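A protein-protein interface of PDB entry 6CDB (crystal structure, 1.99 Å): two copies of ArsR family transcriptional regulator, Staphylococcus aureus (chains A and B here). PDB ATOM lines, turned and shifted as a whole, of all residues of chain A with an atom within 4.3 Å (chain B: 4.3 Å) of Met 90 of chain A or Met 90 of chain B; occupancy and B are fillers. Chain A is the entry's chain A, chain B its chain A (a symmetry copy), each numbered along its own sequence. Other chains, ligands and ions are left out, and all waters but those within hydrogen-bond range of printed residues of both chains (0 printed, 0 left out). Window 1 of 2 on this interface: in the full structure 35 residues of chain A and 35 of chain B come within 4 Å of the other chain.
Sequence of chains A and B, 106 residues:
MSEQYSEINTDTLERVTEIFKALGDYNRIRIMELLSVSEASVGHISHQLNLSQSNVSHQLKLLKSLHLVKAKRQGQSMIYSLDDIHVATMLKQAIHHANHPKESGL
Among the printed residues, merely in contact across the chains: Phe 20 of chain A with Leu 23 of chain B (3.5 Å), Phe 20 of chain A with Ala 94 of chain B (3.7 Å), Leu 23 of chain A with Phe 20 of chain B (3.5 Å), His 86 of chain A with Gln 93 of chain B (3.3 Å), Thr 89 of chain A with Thr 89 of chain B (3.9 Å), Thr 89 of chain A with Gln 93 of chain B (3.8 Å), Met 90 of chain A with Met 90 of chain B (3.6 Å), Met 90 of chain A with Ala 94 of chain B (3.6 Å), Gln 93 of chain A with His 86 of chain B (3.3 Å), Gln 93 of chain A with Thr 89 of chain B (3.8 Å), Ala 94 of chain A with Phe 20 of chain B (3.7 Å) and Ala 94 of chain A with Met 90 of chain B (3.6 Å).
The backbone carbonyl oxygen (O) of Phe 20 of chain B sits close to the backbone carbonyl oxygen (O) of Phe 20 of chain A.
Phe 20 of chain A touches Leu 23 of chain B, and with the chains exchanged Leu 23 of chain A touches Phe 20 of chain B. Phe 20 of chain A touches Ala 94 of chain B, and with the chains exchanged Ala 94 of chain A touches Phe 20 of chain B. His 86 of chain A touches Gln 93 of chain B, and with the chains exchanged Gln 93 of chain A touches His 86 of chain B. Met 90 of chain A touches its own counterpart, Met 90 of chain B. 11 positions are printed for both chains.
Printed residues of chain B within 4 Å of Phe 20 of chain A: Phe 20 (3.1 Å), Leu 23 (3.5 Å) and Ala 94 (3.7 Å). Ala 88 of chain A touches none of the printed residues of chain B. Of the printed residues of chain B, Met 90 of chain A touches Met 90 (3.6 Å) and Ala 94 (3.6 Å). Of the printed residues of chain A, Phe 20 of chain B touches Phe 20 (3.1 Å), Leu 23 (3.5 Å) and Ala 94 (3.7 Å). Of the printed residues of chain A, His 86 of chain B touches Gln 93 (3.3 Å). Val 87 of chain B touches none of the printed residues of chain A. Of the printed residues of chain A, Thr 89 of chain B touches Thr 89 and Gln 93. Met 90 of chain B touches just these residues of chain A: Met 90 (3.6 Å) and Ala 94 (3.6 Å). Printed residues of chain A within 4 Å of Gln 93 of chain B: His 86 (3.3 Å) and Thr 89 (3.8 Å). The nearest printed residue of chain A that does not touch Ala 94 of chain B is His 86 of chain A (5.2 Å).
Printed residues of chain A that touch a printed residue of chain B: Phe 20, Leu 23, His 86, Thr 89, Met 90, Gln 93 and Ala 94. Hydrophobic or aromatic side chains of chain A that line the printed part of chain B: Phe 20, Leu 23, His 86, Met 90 and Ala 94. Along chain A the printed residues that touch a printed residue of chain B span positions 20 to 94. Of the 11 printed residues of chain B, 7 touch a printed residue of chain A. Hydrophobic or aromatic side chains of chain B within 4 Å of the printed part of chain A: Phe 20, Leu 23, His 86, Met 90 and Ala 94. Among the printed residues, 13 pairs touch across the chains. Among the printed residues, no Asp or Glu carboxylate lies within 4 Å of a Lys or Arg side-chain nitrogen of the other chain.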
ATOM      1  N   PHE A  20     -26.639 -18.281  22.401  1.00  0.00           N
ATOM      2  CA  PHE A  20     -28.067 -18.572  22.292  1.00  0.00           C
ATOM      3  C   PHE A  20     -28.832 -18.122  23.534  1.00  0.00           C
ATOM      4  O   PHE A  20     -30.003 -17.732  23.438  1.00  0.00           O
ATOM      5  CB  PHE A  20     -28.283 -20.065  22.048  1.00  0.00           C
ATOM      6  CG  PHE A  20     -27.882 -20.516  20.667  1.00  0.00           C
ATOM      7  CD1 PHE A  20     -28.408 -19.904  19.547  1.00  0.00           C
ATOM      8  CD2 PHE A  20     -26.958 -21.533  20.496  1.00  0.00           C
ATOM      9  CE1 PHE A  20     -28.033 -20.315  18.258  1.00  0.00           C
ATOM     10  CE2 PHE A  20     -26.574 -21.952  19.216  1.00  0.00           C
ATOM     11  CZ  PHE A  20     -27.114 -21.326  18.094  1.00  0.00           C
ATOM     12  N   LEU A  23     -29.413 -14.476  23.071  1.00  0.00           N
ATOM     13  CA  LEU A  23     -30.418 -14.207  22.053  1.00  0.00           C
ATOM     14  C   LEU A  23     -31.798 -14.716  22.436  1.00  0.00           C
ATOM     15  O   LEU A  23     -32.750 -14.471  21.692  1.00  0.00           O
ATOM     16  CB  LEU A  23     -29.999 -14.824  20.711  1.00  0.00           C
ATOM     17  CG  LEU A  23     -28.781 -14.233  20.007  1.00  0.00           C
ATOM     18  CD1 LEU A  23     -28.362 -15.143  18.874  1.00  0.00           C
ATOM     19  CD2 LEU A  23     -29.106 -12.826  19.476  1.00  0.00           C
ATOM     20  N   HIS A  86     -21.398 -14.267   9.918  1.00  0.00           N
ATOM     21  CA  HIS A  86     -21.910 -15.448  10.608  1.00  0.00           C
ATOM     22  C   HIS A  86     -23.111 -15.096  11.474  1.00  0.00           C
ATOM     23  O   HIS A  86     -24.079 -15.863  11.548  1.00  0.00           O
ATOM     24  CB  HIS A  86     -20.809 -16.091  11.455  1.00  0.00           C
ATOM     25  CG  HIS A  86     -19.514 -16.242  10.720  1.00  0.00           C
ATOM     26  ND1 HIS A  86     -18.348 -15.632  11.128  1.00  0.00           N
ATOM     27  CD2 HIS A  86     -19.216 -16.892   9.569  1.00  0.00           C
ATOM     28  CE1 HIS A  86     -17.378 -15.923  10.279  1.00  0.00           C
ATOM     29  NE2 HIS A  86     -17.881 -16.680   9.321  1.00  0.00           N
ATOM     30  N   VAL A  87     -23.056 -13.946  12.141  1.00  0.00           N
ATOM     31  CA  VAL A  87     -24.172 -13.519  12.982  1.00  0.00           C
ATOM     32  C   VAL A  87     -25.393 -13.206  12.125  1.00  0.00           C
ATOM     33  O   VAL A  87     -26.505 -13.674  12.410  1.00  0.00           O
ATOM     34  CB  VAL A  87     -23.747 -12.322  13.850  1.00  0.00           C
ATOM     35  CG1 VAL A  87     -24.899 -11.872  14.761  1.00  0.00           C
ATOM     36  CG2 VAL A  87     -22.529 -12.696  14.689  1.00  0.00           C
ATOM     37  N   ALA A  88     -25.197 -12.453  11.032  1.00  0.00           N
ATOM     38  CA  ALA A  88     -26.303 -12.169  10.121  1.00  0.00           C
ATOM     39  C   ALA A  88     -26.900 -13.452   9.568  1.00  0.00           C
ATOM     40  O   ALA A  88     -28.130 -13.589   9.478  1.00  0.00           O
ATOM     41  CB  ALA A  88     -25.838 -11.260   8.978  1.00  0.00           C
ATOM     42  N   THR A  89     -26.047 -14.408   9.194  1.00  0.00           N
ATOM     43  CA  THR A  89     -26.553 -15.626   8.580  1.00  0.00           C
ATOM     44  C   THR A  89     -27.325 -16.453   9.598  1.00  0.00           C
ATOM     45  O   THR A  89     -28.457 -16.876   9.336  1.00  0.00           O
ATOM     46  CB  THR A  89     -25.410 -16.437   7.965  1.00  0.00           C
ATOM     47  OG1 THR A  89     -24.791 -15.684   6.902  1.00  0.00           O
ATOM     48  CG2 THR A  89     -25.942 -17.737   7.404  1.00  0.00           C
ATOM     49  N   MET A  90     -26.728 -16.682  10.772  1.00  0.00           N
ATOM     50  CA  MET A  90     -27.428 -17.351  11.867  1.00  0.00           C
ATOM     51  C   MET A  90     -28.827 -16.775  12.077  1.00  0.00           C
ATOM     52  O   MET A  90     -29.826 -17.514  12.094  1.00  0.00           O
ATOM     53  CB  MET A  90     -26.594 -17.222  13.141  1.00  0.00           C
ATOM     54  CG  MET A  90     -27.204 -17.855  14.388  1.00  0.00           C
ATOM     55  SD  MET A  90     -26.296 -17.328  15.854  1.00  0.00           S
ATOM     56  CE  MET A  90     -24.739 -16.873  15.096  1.00  0.00           C
ATOM     57  N   LEU A  91     -28.916 -15.445  12.207  1.00  0.00           N
ATOM     58  CA  LEU A  91     -30.191 -14.802  12.533  1.00  0.00           C
ATOM     59  C   LEU A  91     -31.207 -14.935  11.404  1.00  0.00           C
ATOM     60  O   LEU A  91     -32.357 -15.336  11.638  1.00  0.00           O
ATOM     61  CB  LEU A  91     -29.965 -13.327  12.854  1.00  0.00           C
ATOM     62  CG  LEU A  91     -31.217 -12.604  13.338  1.00  0.00           C
ATOM     63  CD1 LEU A  91     -31.595 -13.066  14.751  1.00  0.00           C
ATOM     64  CD2 LEU A  91     -31.023 -11.091  13.253  1.00  0.00           C
ATOM     65  N   LYS A  92     -30.811 -14.569  10.176  1.00  0.00           N
ATOM     66  CA  LYS A  92     -31.735 -14.636   9.039  1.00  0.00           C
ATOM     67  C   LYS A  92     -32.169 -16.071   8.735  1.00  0.00           C
ATOM     68  O   LYS A  92     -33.324 -16.304   8.355  1.00  0.00           O
ATOM     69  CB  LYS A  92     -31.102 -13.976   7.800  1.00  0.00           C
ATOM     70  CG  LYS A  92     -31.074 -12.443   7.900  1.00  0.00           C
ATOM     71  CD  LYS A  92     -30.169 -11.784   6.860  1.00  0.00           C
ATOM     72  CE  LYS A  92     -30.249 -10.263   6.998  1.00  0.00           C
ATOM     73  NZ  LYS A  92     -29.010  -9.578   6.521  1.00  0.00           N
ATOM     74  N   GLN A  93     -31.265 -17.050   8.884  1.00  0.00           N
ATOM     75  CA  GLN A  93     -31.675 -18.440   8.700  1.00  0.00           C
ATOM     76  C   GLN A  93     -32.701 -18.847   9.745  1.00  0.00           C
ATOM     77  O   GLN A  93     -33.682 -19.531   9.425  1.00  0.00           O
ATOM     78  CB  GLN A  93     -30.469 -19.387   8.749  1.00  0.00           C
ATOM     79  CG  GLN A  93     -29.472 -19.179   7.581  1.00  0.00           C
ATOM     80  CD  GLN A  93     -29.876 -19.904   6.305  1.00  0.00           C
ATOM     81  OE1 GLN A  93     -30.331 -21.048   6.349  1.00  0.00           O
ATOM     82  NE2 GLN A  93     -29.701 -19.237   5.153  1.00  0.00           N
ATOM     83  N   ALA A  94     -32.490 -18.436  11.004  1.00  0.00           N
ATOM     84  CA  ALA A  94     -33.474 -18.733  12.049  1.00  0.00           C
ATOM     85  C   ALA A  94     -34.828 -18.083  11.752  1.00  0.00           C
ATOM     86  O   ALA A  94     -35.877 -18.723  11.904  1.00  0.00           O
ATOM     87  CB  ALA A  94     -32.947 -18.277  13.409  1.00  0.00           C
ATOM     88  N   PHE B  20     -34.281 -19.600  20.111  1.00  0.00           N
ATOM     89  CA  PHE B  20     -33.031 -19.279  20.797  1.00  0.00           C
ATOM     90  C   PHE B  20     -33.111 -19.585  22.290  1.00  0.00           C
ATOM     91  O   PHE B  20     -32.101 -19.947  22.907  1.00  0.00           O
ATOM     92  CB  PHE B  20     -32.671 -17.810  20.575  1.00  0.00           C
ATOM     93  CG  PHE B  20     -32.213 -17.505  19.171  1.00  0.00           C
ATOM     94  CD1 PHE B  20     -31.166 -18.205  18.606  1.00  0.00           C
ATOM     95  CD2 PHE B  20     -32.850 -16.537  18.415  1.00  0.00           C
ATOM     96  CE1 PHE B  20     -30.739 -17.932  17.298  1.00  0.00           C
ATOM     97  CE2 PHE B  20     -32.434 -16.254  17.107  1.00  0.00           C
ATOM     98  CZ  PHE B  20     -31.376 -16.968  16.549  1.00  0.00           C
ATOM     99  N   LEU B  23     -32.478 -23.240  22.585  1.00  0.00           N
ATOM    100  CA  LEU B  23     -31.083 -23.575  22.340  1.00  0.00           C
ATOM    101  C   LEU B  23     -30.143 -22.991  23.382  1.00  0.00           C
ATOM    102  O   LEU B  23     -28.945 -23.278  23.330  1.00  0.00           O
ATOM    103  CB  LEU B  23     -30.656 -23.101  20.943  1.00  0.00           C
ATOM    104  CG  LEU B  23     -31.284 -23.794  19.736  1.00  0.00           C
ATOM    105  CD1 LEU B  23     -30.966 -23.008  18.484  1.00  0.00           C
ATOM    106  CD2 LEU B  23     -30.759 -25.234  19.618  1.00  0.00           C
ATOM    107  N   HIS B  86     -31.710 -24.943   7.295  1.00  0.00           N
ATOM    108  CA  HIS B  86     -31.640 -23.687   8.036  1.00  0.00           C
ATOM    109  C   HIS B  86     -31.145 -23.919   9.457  1.00  0.00           C
ATOM    110  O   HIS B  86     -30.365 -23.120   9.989  1.00  0.00           O
ATOM    111  CB  HIS B  86     -33.008 -22.999   8.052  1.00  0.00           C
ATOM    112  CG  HIS B  86     -33.660 -22.958   6.705  1.00  0.00           C
ATOM    113  ND1 HIS B  86     -34.871 -23.560   6.443  1.00  0.00           N
ATOM    114  CD2 HIS B  86     -33.240 -22.430   5.530  1.00  0.00           C
ATOM    115  CE1 HIS B  86     -35.186 -23.380   5.172  1.00  0.00           C
ATOM    116  NE2 HIS B  86     -34.210 -22.704   4.596  1.00  0.00           N
ATOM    117  N   VAL B  87     -31.600 -25.001  10.084  1.00  0.00           N
ATOM    118  CA  VAL B  87     -31.163 -25.313  11.443  1.00  0.00           C
ATOM    119  C   VAL B  87     -29.681 -25.670  11.456  1.00  0.00           C
ATOM    120  O   VAL B  87     -28.909 -25.144  12.271  1.00  0.00           O
ATOM    121  CB  VAL B  87     -32.038 -26.433  12.031  1.00  0.00           C
ATOM    122  CG1 VAL B  87     -31.611 -26.759  13.471  1.00  0.00           C
ATOM    123  CG2 VAL B  87     -33.505 -26.016  12.000  1.00  0.00           C
ATOM    124  N   ALA B  88     -29.251 -26.530  10.520  1.00  0.00           N
ATOM    125  CA  ALA B  88     -27.833 -26.867  10.422  1.00  0.00           C
ATOM    126  C   ALA B  88     -26.991 -25.626  10.179  1.00  0.00           C
ATOM    127  O   ALA B  88     -25.920 -25.461  10.784  1.00  0.00           O
ATOM    128  CB  ALA B  88     -27.601 -27.894   9.309  1.00  0.00           C
ATOM    129  N   THR B  89     -27.457 -24.735   9.301  1.00  0.00           N
ATOM    130  CA  THR B  89     -26.657 -23.567   8.965  1.00  0.00           C
ATOM    131  C   THR B  89     -26.568 -22.624  10.156  1.00  0.00           C
ATOM    132  O   THR B  89     -25.473 -22.195  10.537  1.00  0.00           O
ATOM    133  CB  THR B  89     -27.233 -22.853   7.740  1.00  0.00           C
ATOM    134  OG1 THR B  89     -27.168 -23.722   6.591  1.00  0.00           O
ATOM    135  CG2 THR B  89     -26.439 -21.597   7.454  1.00  0.00           C
ATOM    136  N   MET B  90     -27.715 -22.302  10.763  1.00  0.00           N
ATOM    137  CA  MET B  90     -27.732 -21.510  11.991  1.00  0.00           C
ATOM    138  C   MET B  90     -26.711 -22.022  13.006  1.00  0.00           C
ATOM    139  O   MET B  90     -25.874 -21.256  13.511  1.00  0.00           O
ATOM    140  CB  MET B  90     -29.142 -21.541  12.582  1.00  0.00           C
ATOM    141  CG  MET B  90     -29.320 -20.774  13.888  1.00  0.00           C
ATOM    142  SD  MET B  90     -30.910 -21.184  14.632  1.00  0.00           S
ATOM    143  CE  MET B  90     -31.784 -21.756  13.177  1.00  0.00           C
ATOM    144  N   LEU B  91     -26.750 -23.330  13.291  1.00  0.00           N
ATOM    145  CA  LEU B  91     -25.899 -23.901  14.337  1.00  0.00           C
ATOM    146  C   LEU B  91     -24.421 -23.847  13.968  1.00  0.00           C
ATOM    147  O   LEU B  91     -23.590 -23.391  14.768  1.00  0.00           O
ATOM    148  CB  LEU B  91     -26.310 -25.344  14.615  1.00  0.00           C
ATOM    149  CG  LEU B  91     -25.569 -25.980  15.786  1.00  0.00           C
ATOM    150  CD1 LEU B  91     -26.037 -25.374  17.114  1.00  0.00           C
ATOM    151  CD2 LEU B  91     -25.726 -27.500  15.751  1.00  0.00           C
ATOM    152  N   LYS B  92     -24.068 -24.340  12.772  1.00  0.00           N
ATOM    153  CA  LYS B  92     -22.663 -24.355  12.351  1.00  0.00           C
ATOM    154  C   LYS B  92     -22.091 -22.944  12.208  1.00  0.00           C
ATOM    155  O   LYS B  92     -20.916 -22.713  12.524  1.00  0.00           O
ATOM    156  CB  LYS B  92     -22.509 -25.150  11.041  1.00  0.00           C
ATOM    157  CG  LYS B  92     -22.633 -26.665  11.254  1.00  0.00           C
ATOM    158  CD  LYS B  92     -22.816 -27.448   9.954  1.00  0.00           C
ATOM    159  CE  LYS B  92     -22.872 -28.945  10.258  1.00  0.00           C
ATOM    160  NZ  LYS B  92     -23.648 -29.709   9.235  1.00  0.00           N
ATOM    161  N   GLN B  93     -22.892 -21.981  11.728  1.00  0.00           N
ATOM    162  CA  GLN B  93     -22.409 -20.605  11.675  1.00  0.00           C
ATOM    163  C   GLN B  93     -22.137 -20.069  13.071  1.00  0.00           C
ATOM    164  O   GLN B  93     -21.126 -19.391  13.294  1.00  0.00           O
ATOM    165  CB  GLN B  93     -23.405 -19.693  10.946  1.00  0.00           C
ATOM    166  CG  GLN B  93     -23.579 -20.041   9.446  1.00  0.00           C
ATOM    167  CD  GLN B  93     -22.506 -19.430   8.556  1.00  0.00           C
ATOM    168  OE1 GLN B  93     -22.121 -18.275   8.738  1.00  0.00           O
ATOM    169  NE2 GLN B  93     -22.023 -20.210   7.575  1.00  0.00           N
ATOM    170  N   ALA B  94     -23.032 -20.363  14.026  1.00  0.00           N
ATOM    171  CA  ALA B  94     -22.797 -19.939  15.409  1.00  0.00           C
ATOM    172  C   ALA B  94     -21.531 -20.574  15.988  1.00  0.00           C
ATOM    173  O   ALA B  94     -20.731 -19.892  16.642  1.00  0.00           O
ATOM    174  CB  ALA B  94     -24.012 -20.279  16.274  1.00  0.00           C
